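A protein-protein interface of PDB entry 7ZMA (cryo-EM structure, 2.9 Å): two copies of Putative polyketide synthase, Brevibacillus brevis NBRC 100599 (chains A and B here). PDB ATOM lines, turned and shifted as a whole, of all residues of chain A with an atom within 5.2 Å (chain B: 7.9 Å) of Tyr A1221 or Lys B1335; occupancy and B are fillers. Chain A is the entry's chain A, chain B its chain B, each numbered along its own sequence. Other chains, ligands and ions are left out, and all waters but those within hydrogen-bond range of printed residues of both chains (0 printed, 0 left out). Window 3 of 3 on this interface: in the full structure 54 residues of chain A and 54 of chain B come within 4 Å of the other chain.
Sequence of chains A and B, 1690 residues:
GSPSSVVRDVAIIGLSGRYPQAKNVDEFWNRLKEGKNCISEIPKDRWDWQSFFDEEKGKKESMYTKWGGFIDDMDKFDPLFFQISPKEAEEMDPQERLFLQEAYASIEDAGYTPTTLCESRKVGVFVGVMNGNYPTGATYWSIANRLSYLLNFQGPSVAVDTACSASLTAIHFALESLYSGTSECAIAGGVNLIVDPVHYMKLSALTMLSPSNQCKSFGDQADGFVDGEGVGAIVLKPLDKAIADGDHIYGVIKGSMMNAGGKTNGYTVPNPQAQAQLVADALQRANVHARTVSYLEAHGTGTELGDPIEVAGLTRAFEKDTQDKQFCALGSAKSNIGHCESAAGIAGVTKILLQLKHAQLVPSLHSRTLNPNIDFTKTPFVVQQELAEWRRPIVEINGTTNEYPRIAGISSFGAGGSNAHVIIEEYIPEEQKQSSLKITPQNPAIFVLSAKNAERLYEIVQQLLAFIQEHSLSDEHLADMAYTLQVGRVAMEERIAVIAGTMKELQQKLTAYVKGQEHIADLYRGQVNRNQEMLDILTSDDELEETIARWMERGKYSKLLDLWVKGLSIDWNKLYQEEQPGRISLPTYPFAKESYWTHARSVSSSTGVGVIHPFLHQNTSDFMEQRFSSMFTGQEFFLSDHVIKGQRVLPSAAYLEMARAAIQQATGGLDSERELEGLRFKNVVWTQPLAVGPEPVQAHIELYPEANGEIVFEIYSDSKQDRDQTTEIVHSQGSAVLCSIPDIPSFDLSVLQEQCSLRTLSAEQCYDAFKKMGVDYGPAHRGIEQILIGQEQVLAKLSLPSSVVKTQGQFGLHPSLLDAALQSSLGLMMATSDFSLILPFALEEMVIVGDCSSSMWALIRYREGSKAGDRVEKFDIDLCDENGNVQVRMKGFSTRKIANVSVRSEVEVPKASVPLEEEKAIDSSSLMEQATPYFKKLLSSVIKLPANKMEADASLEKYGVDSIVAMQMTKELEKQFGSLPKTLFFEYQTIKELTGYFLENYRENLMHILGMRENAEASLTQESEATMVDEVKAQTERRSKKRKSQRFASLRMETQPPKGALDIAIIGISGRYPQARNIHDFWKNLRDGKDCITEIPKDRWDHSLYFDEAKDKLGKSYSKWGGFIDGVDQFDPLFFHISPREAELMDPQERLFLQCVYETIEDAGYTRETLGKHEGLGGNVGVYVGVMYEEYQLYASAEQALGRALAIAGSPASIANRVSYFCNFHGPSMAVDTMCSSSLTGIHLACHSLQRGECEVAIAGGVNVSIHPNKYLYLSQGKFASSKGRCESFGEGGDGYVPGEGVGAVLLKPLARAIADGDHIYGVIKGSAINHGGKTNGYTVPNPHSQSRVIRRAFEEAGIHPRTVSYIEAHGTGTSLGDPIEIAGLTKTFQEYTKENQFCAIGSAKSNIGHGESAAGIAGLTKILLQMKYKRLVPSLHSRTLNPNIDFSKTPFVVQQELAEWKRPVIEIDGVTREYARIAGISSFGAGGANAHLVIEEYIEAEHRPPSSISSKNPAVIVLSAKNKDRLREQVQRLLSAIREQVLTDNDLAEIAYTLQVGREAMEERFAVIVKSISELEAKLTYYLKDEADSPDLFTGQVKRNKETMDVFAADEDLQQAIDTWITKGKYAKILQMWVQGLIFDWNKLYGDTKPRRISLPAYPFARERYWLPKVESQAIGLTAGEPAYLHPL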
ATOM      1  N   ALA A1216      26.789 -17.660  24.755  1.00  0.00           N
ATOM      2  CA  ALA A1216      27.436 -16.919  25.830  1.00  0.00           C
ATOM      3  C   ALA A1216      27.066 -15.445  25.847  1.00  0.00           C
ATOM      4  O   ALA A1216      26.997 -14.842  26.926  1.00  0.00           O
ATOM      5  CB  ALA A1216      28.957 -17.046  25.714  1.00  0.00           C
ATOM      6  N   ASN A1217      26.830 -14.852  24.676  1.00  0.00           N
ATOM      7  CA  ASN A1217      26.491 -13.436  24.621  1.00  0.00           C
ATOM      8  C   ASN A1217      25.142 -13.166  25.272  1.00  0.00           C
ATOM      9  O   ASN A1217      24.978 -12.159  25.968  1.00  0.00           O
ATOM     10  CB  ASN A1217      26.505 -12.958  23.170  1.00  0.00           C
ATOM     11  CG  ASN A1217      27.909 -12.812  22.623  1.00  0.00           C
ATOM     12  OD1 ASN A1217      28.891 -13.058  23.324  1.00  0.00           O
ATOM     13  ND2 ASN A1217      28.015 -12.416  21.363  1.00  0.00           N
ATOM     14  N   ARG A1218      24.164 -14.049  25.062  1.00  0.00           N
ATOM     15  CA  ARG A1218      22.871 -13.892  25.717  1.00  0.00           C
ATOM     16  C   ARG A1218      23.011 -13.993  27.229  1.00  0.00           C
ATOM     17  O   ARG A1218      22.370 -13.242  27.973  1.00  0.00           O
ATOM     18  CB  ARG A1218      21.894 -14.942  25.192  1.00  0.00           C
ATOM     19  CG  ARG A1218      20.496 -14.863  25.782  1.00  0.00           C
ATOM     20  CD  ARG A1218      19.685 -13.746  25.156  1.00  0.00           C
ATOM     21  NE  ARG A1218      19.255 -14.071  23.802  1.00  0.00           N
ATOM     22  CZ  ARG A1218      18.332 -13.398  23.130  1.00  0.00           C
ATOM     23  NH1 ARG A1218      17.717 -12.352  23.656  1.00  0.00           N
ATOM     24  NH2 ARG A1218      18.018 -13.786  21.897  1.00  0.00           N
ATOM     25  N   VAL A1219      23.838 -14.926  27.704  1.00  0.00           N
ATOM     26  CA  VAL A1219      24.063 -15.060  29.139  1.00  0.00           C
ATOM     27  C   VAL A1219      24.660 -13.777  29.700  1.00  0.00           C
ATOM     28  O   VAL A1219      24.190 -13.241  30.714  1.00  0.00           O
ATOM     29  CB  VAL A1219      24.972 -16.272  29.418  1.00  0.00           C
ATOM     30  CG1 VAL A1219      25.320 -16.359  30.895  1.00  0.00           C
ATOM     31  CG2 VAL A1219      24.316 -17.555  28.943  1.00  0.00           C
ATOM     32  N   SER A1220      25.701 -13.263  29.044  1.00  0.00           N
ATOM     33  CA  SER A1220      26.351 -12.050  29.525  1.00  0.00           C
ATOM     34  C   SER A1220      25.412 -10.853  29.466  1.00  0.00           C
ATOM     35  O   SER A1220      25.464  -9.986  30.342  1.00  0.00           O
ATOM     36  CB  SER A1220      27.613 -11.776  28.713  1.00  0.00           C
ATOM     37  OG  SER A1220      28.573 -12.797  28.908  1.00  0.00           O
ATOM     38  N   TYR A1221      24.552 -10.786  28.452  1.00  0.00           N
ATOM     39  CA  TYR A1221      23.610  -9.679  28.343  1.00  0.00           C
ATOM     40  C   TYR A1221      22.555  -9.743  29.441  1.00  0.00           C
ATOM     41  O   TYR A1221      22.260  -8.733  30.090  1.00  0.00           O
ATOM     42  CB  TYR A1221      22.961  -9.696  26.960  1.00  0.00           C
ATOM     43  CG  TYR A1221      21.633  -8.986  26.878  1.00  0.00           C
ATOM     44  CD1 TYR A1221      21.567  -7.607  26.756  1.00  0.00           C
ATOM     45  CD2 TYR A1221      20.443  -9.697  26.900  1.00  0.00           C
ATOM     46  CE1 TYR A1221      20.356  -6.956  26.673  1.00  0.00           C
ATOM     47  CE2 TYR A1221      19.225  -9.055  26.818  1.00  0.00           C
ATOM     48  CZ  TYR A1221      19.189  -7.684  26.704  1.00  0.00           C
ATOM     49  OH  TYR A1221      17.978  -7.037  26.622  1.00  0.00           O
ATOM     50  N   PHE A1222      21.973 -10.921  29.663  1.00  0.00           N
ATOM     51  CA  PHE A1222      20.949 -11.054  30.692  1.00  0.00           C
ATOM     52  C   PHE A1222      21.518 -10.770  32.074  1.00  0.00           C
ATOM     53  O   PHE A1222      20.899 -10.068  32.882  1.00  0.00           O
ATOM     54  CB  PHE A1222      20.328 -12.449  30.644  1.00  0.00           C
ATOM     55  CG  PHE A1222      19.404 -12.737  31.794  1.00  0.00           C
ATOM     56  CD1 PHE A1222      18.139 -12.177  31.841  1.00  0.00           C
ATOM     57  CD2 PHE A1222      19.802 -13.566  32.828  1.00  0.00           C
ATOM     58  CE1 PHE A1222      17.291 -12.441  32.898  1.00  0.00           C
ATOM     59  CE2 PHE A1222      18.956 -13.831  33.886  1.00  0.00           C
ATOM     60  CZ  PHE A1222      17.700 -13.267  33.920  1.00  0.00           C
ATOM     61  N   CYS A1223      22.703 -11.305  32.370  1.00  0.00           N
ATOM     62  CA  CYS A1223      23.300 -11.118  33.685  1.00  0.00           C
ATOM     63  C   CYS A1223      24.092  -9.822  33.805  1.00  0.00           C
ATOM     64  O   CYS A1223      24.610  -9.532  34.889  1.00  0.00           O
ATOM     65  CB  CYS A1223      24.196 -12.312  34.018  1.00  0.00           C
ATOM     66  SG  CYS A1223      23.336 -13.902  33.981  1.00  0.00           S
ATOM     67  N   ASN A1224      24.193  -9.040  32.731  1.00  0.00           N
ATOM     68  CA  ASN A1224      24.904  -7.764  32.735  1.00  0.00           C
ATOM     69  C   ASN A1224      26.352  -7.945  33.194  1.00  0.00           C
ATOM     70  O   ASN A1224      26.787  -7.408  34.215  1.00  0.00           O
ATOM     71  CB  ASN A1224      24.173  -6.732  33.597  1.00  0.00           C
ATOM     72  CG  ASN A1224      24.762  -5.346  33.465  1.00  0.00           C
ATOM     73  OD1 ASN A1224      24.587  -4.676  32.448  1.00  0.00           O
ATOM     74  ND2 ASN A1224      25.456  -4.900  34.499  1.00  0.00           N
ATOM     75  N   PHE A1225      27.096  -8.717  32.408  1.00  0.00           N
ATOM     76  CA  PHE A1225      28.517  -8.933  32.630  1.00  0.00           C
ATOM     77  C   PHE A1225      29.328  -8.129  31.622  1.00  0.00           C
ATOM     78  O   PHE A1225      28.936  -7.971  30.463  1.00  0.00           O
ATOM     79  CB  PHE A1225      28.868 -10.418  32.519  1.00  0.00           C
ATOM     80  CG  PHE A1225      28.255 -11.274  33.592  1.00  0.00           C
ATOM     81  CD1 PHE A1225      28.009 -10.765  34.857  1.00  0.00           C
ATOM     82  CD2 PHE A1225      27.932 -12.594  33.338  1.00  0.00           C
ATOM     83  CE1 PHE A1225      27.450 -11.553  35.840  1.00  0.00           C
ATOM     84  CE2 PHE A1225      27.374 -13.386  34.319  1.00  0.00           C
ATOM     85  CZ  PHE A1225      27.134 -12.865  35.571  1.00  0.00           C
ATOM     86  N   HIS B1332      32.684  -7.169  26.917  1.00  0.00           N
ATOM     87  CA  HIS B1332      31.288  -7.269  26.519  1.00  0.00           C
ATOM     88  C   HIS B1332      30.533  -6.081  27.097  1.00  0.00           C
ATOM     89  O   HIS B1332      30.776  -5.681  28.238  1.00  0.00           O
ATOM     90  CB  HIS B1332      30.666  -8.589  26.997  1.00  0.00           C
ATOM     91  CG  HIS B1332      29.345  -8.905  26.365  1.00  0.00           C
ATOM     92  ND1 HIS B1332      29.117 -10.065  25.657  1.00  0.00           N
ATOM     93  CD2 HIS B1332      28.176  -8.226  26.359  1.00  0.00           C
ATOM     94  CE1 HIS B1332      27.868 -10.076  25.226  1.00  0.00           C
ATOM     95  NE2 HIS B1332      27.275  -8.972  25.639  1.00  0.00           N
ATOM     96  N   GLY B1333      29.624  -5.515  26.302  1.00  0.00           N
ATOM     97  CA  GLY B1333      28.919  -4.321  26.743  1.00  0.00           C
ATOM     98  C   GLY B1333      28.081  -4.559  27.984  1.00  0.00           C
ATOM     99  O   GLY B1333      28.236  -3.871  28.996  1.00  0.00           O
ATOM    100  N   GLY B1334      27.177  -5.534  27.921  1.00  0.00           N
ATOM    101  CA  GLY B1334      26.364  -5.897  29.064  1.00  0.00           C
ATOM    102  C   GLY B1334      24.883  -5.725  28.806  1.00  0.00           C
ATOM    103  O   GLY B1334      24.414  -5.934  27.683  1.00  0.00           O
ATOM    104  N   LYS B1335      24.135  -5.345  29.837  1.00  0.00           N
ATOM    105  CA  LYS B1335      22.701  -5.120  29.715  1.00  0.00           C
ATOM    106  C   LYS B1335      22.466  -3.700  29.214  1.00  0.00           C
ATOM    107  O   LYS B1335      22.913  -2.733  29.841  1.00  0.00           O
ATOM    108  CB  LYS B1335      22.001  -5.351  31.053  1.00  0.00           C
ATOM    109  CG  LYS B1335      20.528  -4.979  31.076  1.00  0.00           C
ATOM    110  CD  LYS B1335      19.728  -5.756  30.054  1.00  0.00           C
ATOM    111  CE  LYS B1335      18.262  -5.375  30.109  1.00  0.00           C
ATOM    112  NZ  LYS B1335      17.478  -5.997  29.011  1.00  0.00           N
ATOM    113  N   THR B1336      21.768  -3.580  28.089  1.00  0.00           N
ATOM    114  CA  THR B1336      21.477  -2.302  27.460  1.00  0.00           C
ATOM    115  C   THR B1336      19.975  -2.199  27.222  1.00  0.00           C
ATOM    116  O   THR B1336      19.196  -3.062  27.635  1.00  0.00           O
ATOM    117  CB  THR B1336      22.251  -2.144  26.146  1.00  0.00           C
ATOM    118  OG1 THR B1336      21.939  -3.235  25.270  1.00  0.00           O
ATOM    119  CG2 THR B1336      23.746  -2.124  26.408  1.00  0.00           C
ATOM    120  N   ASN B1337      19.566  -1.128  26.540  1.00  0.00           N
ATOM    121  CA  ASN B1337      18.157  -0.901  26.222  1.00  0.00           C
ATOM    122  C   ASN B1337      17.750  -1.742  25.010  1.00  0.00           C
ATOM    123  O   ASN B1337      17.302  -1.241  23.978  1.00  0.00           O
ATOM    124  CB  ASN B1337      17.904   0.581  25.980  1.00  0.00           C
ATOM    125  CG  ASN B1337      16.428   0.925  25.968  1.00  0.00           C
ATOM    126  OD1 ASN B1337      15.573   0.049  26.104  1.00  0.00           O
ATOM    127  ND2 ASN B1337      16.120   2.207  25.806  1.00  0.00           N
ATOM    128  N   GLY B1338      17.918  -3.047  25.158  1.00  0.00           N
ATOM    129  CA  GLY B1338      17.621  -4.002  24.110  1.00  0.00           C
ATOM    130  C   GLY B1338      18.858  -4.763  23.668  1.00  0.00           C
ATOM    131  O   GLY B1338      19.996  -4.388  23.948  1.00  0.00           O
ATOM    132  N   TYR B1339      18.601  -5.858  22.964  1.00  0.00           N
ATOM    133  CA  TYR B1339      19.657  -6.690  22.416  1.00  0.00           C
ATOM    134  C   TYR B1339      20.199  -6.068  21.136  1.00  0.00           C
ATOM    135  O   TYR B1339      19.484  -5.373  20.409  1.00  0.00           O
ATOM    136  CB  TYR B1339      19.138  -8.103  22.139  1.00  0.00           C
ATOM    137  CG  TYR B1339      20.205  -9.179  22.111  1.00  0.00           C
ATOM    138  CD1 TYR B1339      21.164  -9.264  23.112  1.00  0.00           C
ATOM    139  CD2 TYR B1339      20.242 -10.120  21.092  1.00  0.00           C
ATOM    140  CE1 TYR B1339      22.134 -10.247  23.092  1.00  0.00           C
ATOM    141  CE2 TYR B1339      21.209 -11.107  21.065  1.00  0.00           C
ATOM    142  CZ  TYR B1339      22.151 -11.165  22.068  1.00  0.00           C
ATOM    143  OH  TYR B1339      23.115 -12.144  22.045  1.00  0.00           O
ATOM    144  N   THR B1340      21.476  -6.329  20.864  1.00  0.00           N
ATOM    145  CA  THR B1340      22.150  -5.780  19.688  1.00  0.00           C
ATOM    146  C   THR B1340      22.172  -4.254  19.725  1.00  0.00           C
ATOM    147  O   THR B1340      21.887  -3.585  18.731  1.00  0.00           O
ATOM    148  CB  THR B1340      21.499  -6.274  18.394  1.00  0.00           C
ATOM    149  OG1 THR B1340      20.324  -5.501  18.117  1.00  0.00           O
ATOM    150  CG2 THR B1340      21.124  -7.743  18.506  1.00  0.00           C
ATOM    151  N   VAL B1341      22.515  -3.698  20.889  1.00  0.00           N
ATOM    152  CA  VAL B1341      22.645  -2.260  21.069  1.00  0.00           C
ATOM    153  C   VAL B1341      24.009  -1.993  21.695  1.00  0.00           C
ATOM    154  O   VAL B1341      24.265  -2.424  22.823  1.00  0.00           O
ATOM    155  CB  VAL B1341      21.526  -1.677  21.950  1.00  0.00           C
ATOM    156  CG1 VAL B1341      21.686  -0.173  22.095  1.00  0.00           C
ATOM    157  CG2 VAL B1341      20.170  -2.010  21.361  1.00  0.00           C
ATOM    158  N   ASN B1343      27.291  -0.323  23.604  1.00  0.00           N
ATOM    159  CA  ASN B1343      27.436   0.451  24.836  1.00  0.00           C
ATOM    160  C   ASN B1343      28.668   1.346  24.752  1.00  0.00           C
ATOM    161  O   ASN B1343      29.806   0.843  24.845  1.00  0.00           O
ATOM    162  CB  ASN B1343      27.528  -0.480  26.044  1.00  0.00           C
ATOM    163  CG  ASN B1343      27.315   0.246  27.356  1.00  0.00           C
ATOM    164  OD1 ASN B1343      27.242   1.474  27.396  1.00  0.00           O
ATOM    165  ND2 ASN B1343      27.198  -0.513  28.437  1.00  0.00           N
ATOM    166  N   GLY B1488      26.323  -9.137  19.212  1.00  0.00           N
ATOM    167  CA  GLY B1488      25.896  -9.631  20.508  1.00  0.00           C
ATOM    168  C   GLY B1488      26.286  -8.716  21.650  1.00  0.00           C
ATOM    169  O   GLY B1488      25.546  -8.586  22.628  1.00  0.00           O
ATOM    170  N   GLY B1489      27.445  -8.074  21.546  1.00  0.00           N
ATOM    171  CA  GLY B1489      27.918  -7.179  22.581  1.00  0.00           C
ATOM    172  C   GLY B1489      29.411  -7.280  22.797  1.00  0.00           C
ATOM    173  O   GLY B1489      30.006  -6.446  23.486  1.00  0.00           O
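Printed residues of chain B within 4 Å of Arg A1218: Tyr B1339 (3.7 Å). Tyr A1221 touches just these residues of chain B: Gly B1334, Lys B1335, Thr B1336, Gly B1338 and Tyr B1339. Cys A1223 touches none of the printed residues of chain B. Of the printed residues of chain B, Asn A1224 touches Gly B1334 and Lys B1335. Lys B1335 touches just these residues of chain A: Tyr A1221 (2.7 Å) and Asn A1224 (2.7 Å). Asn B1343 touches none of the printed residues of chain A. Of the printed residues of chain A, Gly B1488 touches Asn A1217 (3.6 Å). The nearest residue of chain B that does not touch Tyr A1221 is His B1332 (4.3 Å). The nearest residue of chain A that does not touch Lys B1335 is Ser A1220 (4.9 Å).
No position is printed for both chains.
The side-chain hydroxyl (OH) of Tyr A1221 sits at hydrogen-bond distance from the side-chain amino group (NZ) of Lys B1335 (2.7 Å). N of Lys B1335 is in hydrogen-bond range of OD1 of Asn A1224.
Hydrophobic or aromatic side chains of chain B that line the printed part of chain A: His B1332 and Tyr B1339. Along chain B the printed residues that touch a printed residue of chain A span positions 1332 to 1488. Hydrophobic or aromatic side chains of chain A that line the printed part of chain B: Tyr A1221. Among the printed residues, no Asp or Glu carboxylate lies within 4 Å of a Lys or Arg side-chain nitrogen of the other chain.
The backbone carbonyl oxygen of Ala A1216 lies within hydrogen-bond range of the side-chain hydroxyl of Ser A1220. The backbone carbonyl oxygen (O) of Ser A1220 lies within hydrogen-bond range of the backbone NH (N) of Phe A1225, 2.9 Å away. The backbone carbonyl oxygen (O) of Gly B1488 is in hydrogen-bond range of a ring nitrogen (NE2) of His B1332 (3.5 Å). OG1 of Thr B1336 is in hydrogen-bond range of O of Gly B1338, 2.6 Å away. OG1 of Thr B1336 lies within hydrogen-bond range of O of Val B1341, 3.5 Å away.
Among the printed residues, merely in contact across the chains: Tyr A1221 with Gly B1334 (3.4 Å), Phe A1225 with Gly B1334 (3.6 Å), Asn A1217 with Gly B1488 (3.6 Å), Asn A1217 with His B1332 (3.6 Å), Asn A1217 with Tyr B1339 (3.7 Å), Phe A1225 with His B1332 (3.7 Å), Arg A1218 with Tyr B1339 (3.7 Å), Tyr A1221 with Gly B1338 (3.8 Å), Asn A1224 with Gly B1334 (3.8 Å), Tyr A1221 with Tyr B1339 (3.8 Å), Ser A1220 with His B1332 (3.8 Å) and Tyr A1221 with Thr B1336 (3.9 Å).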
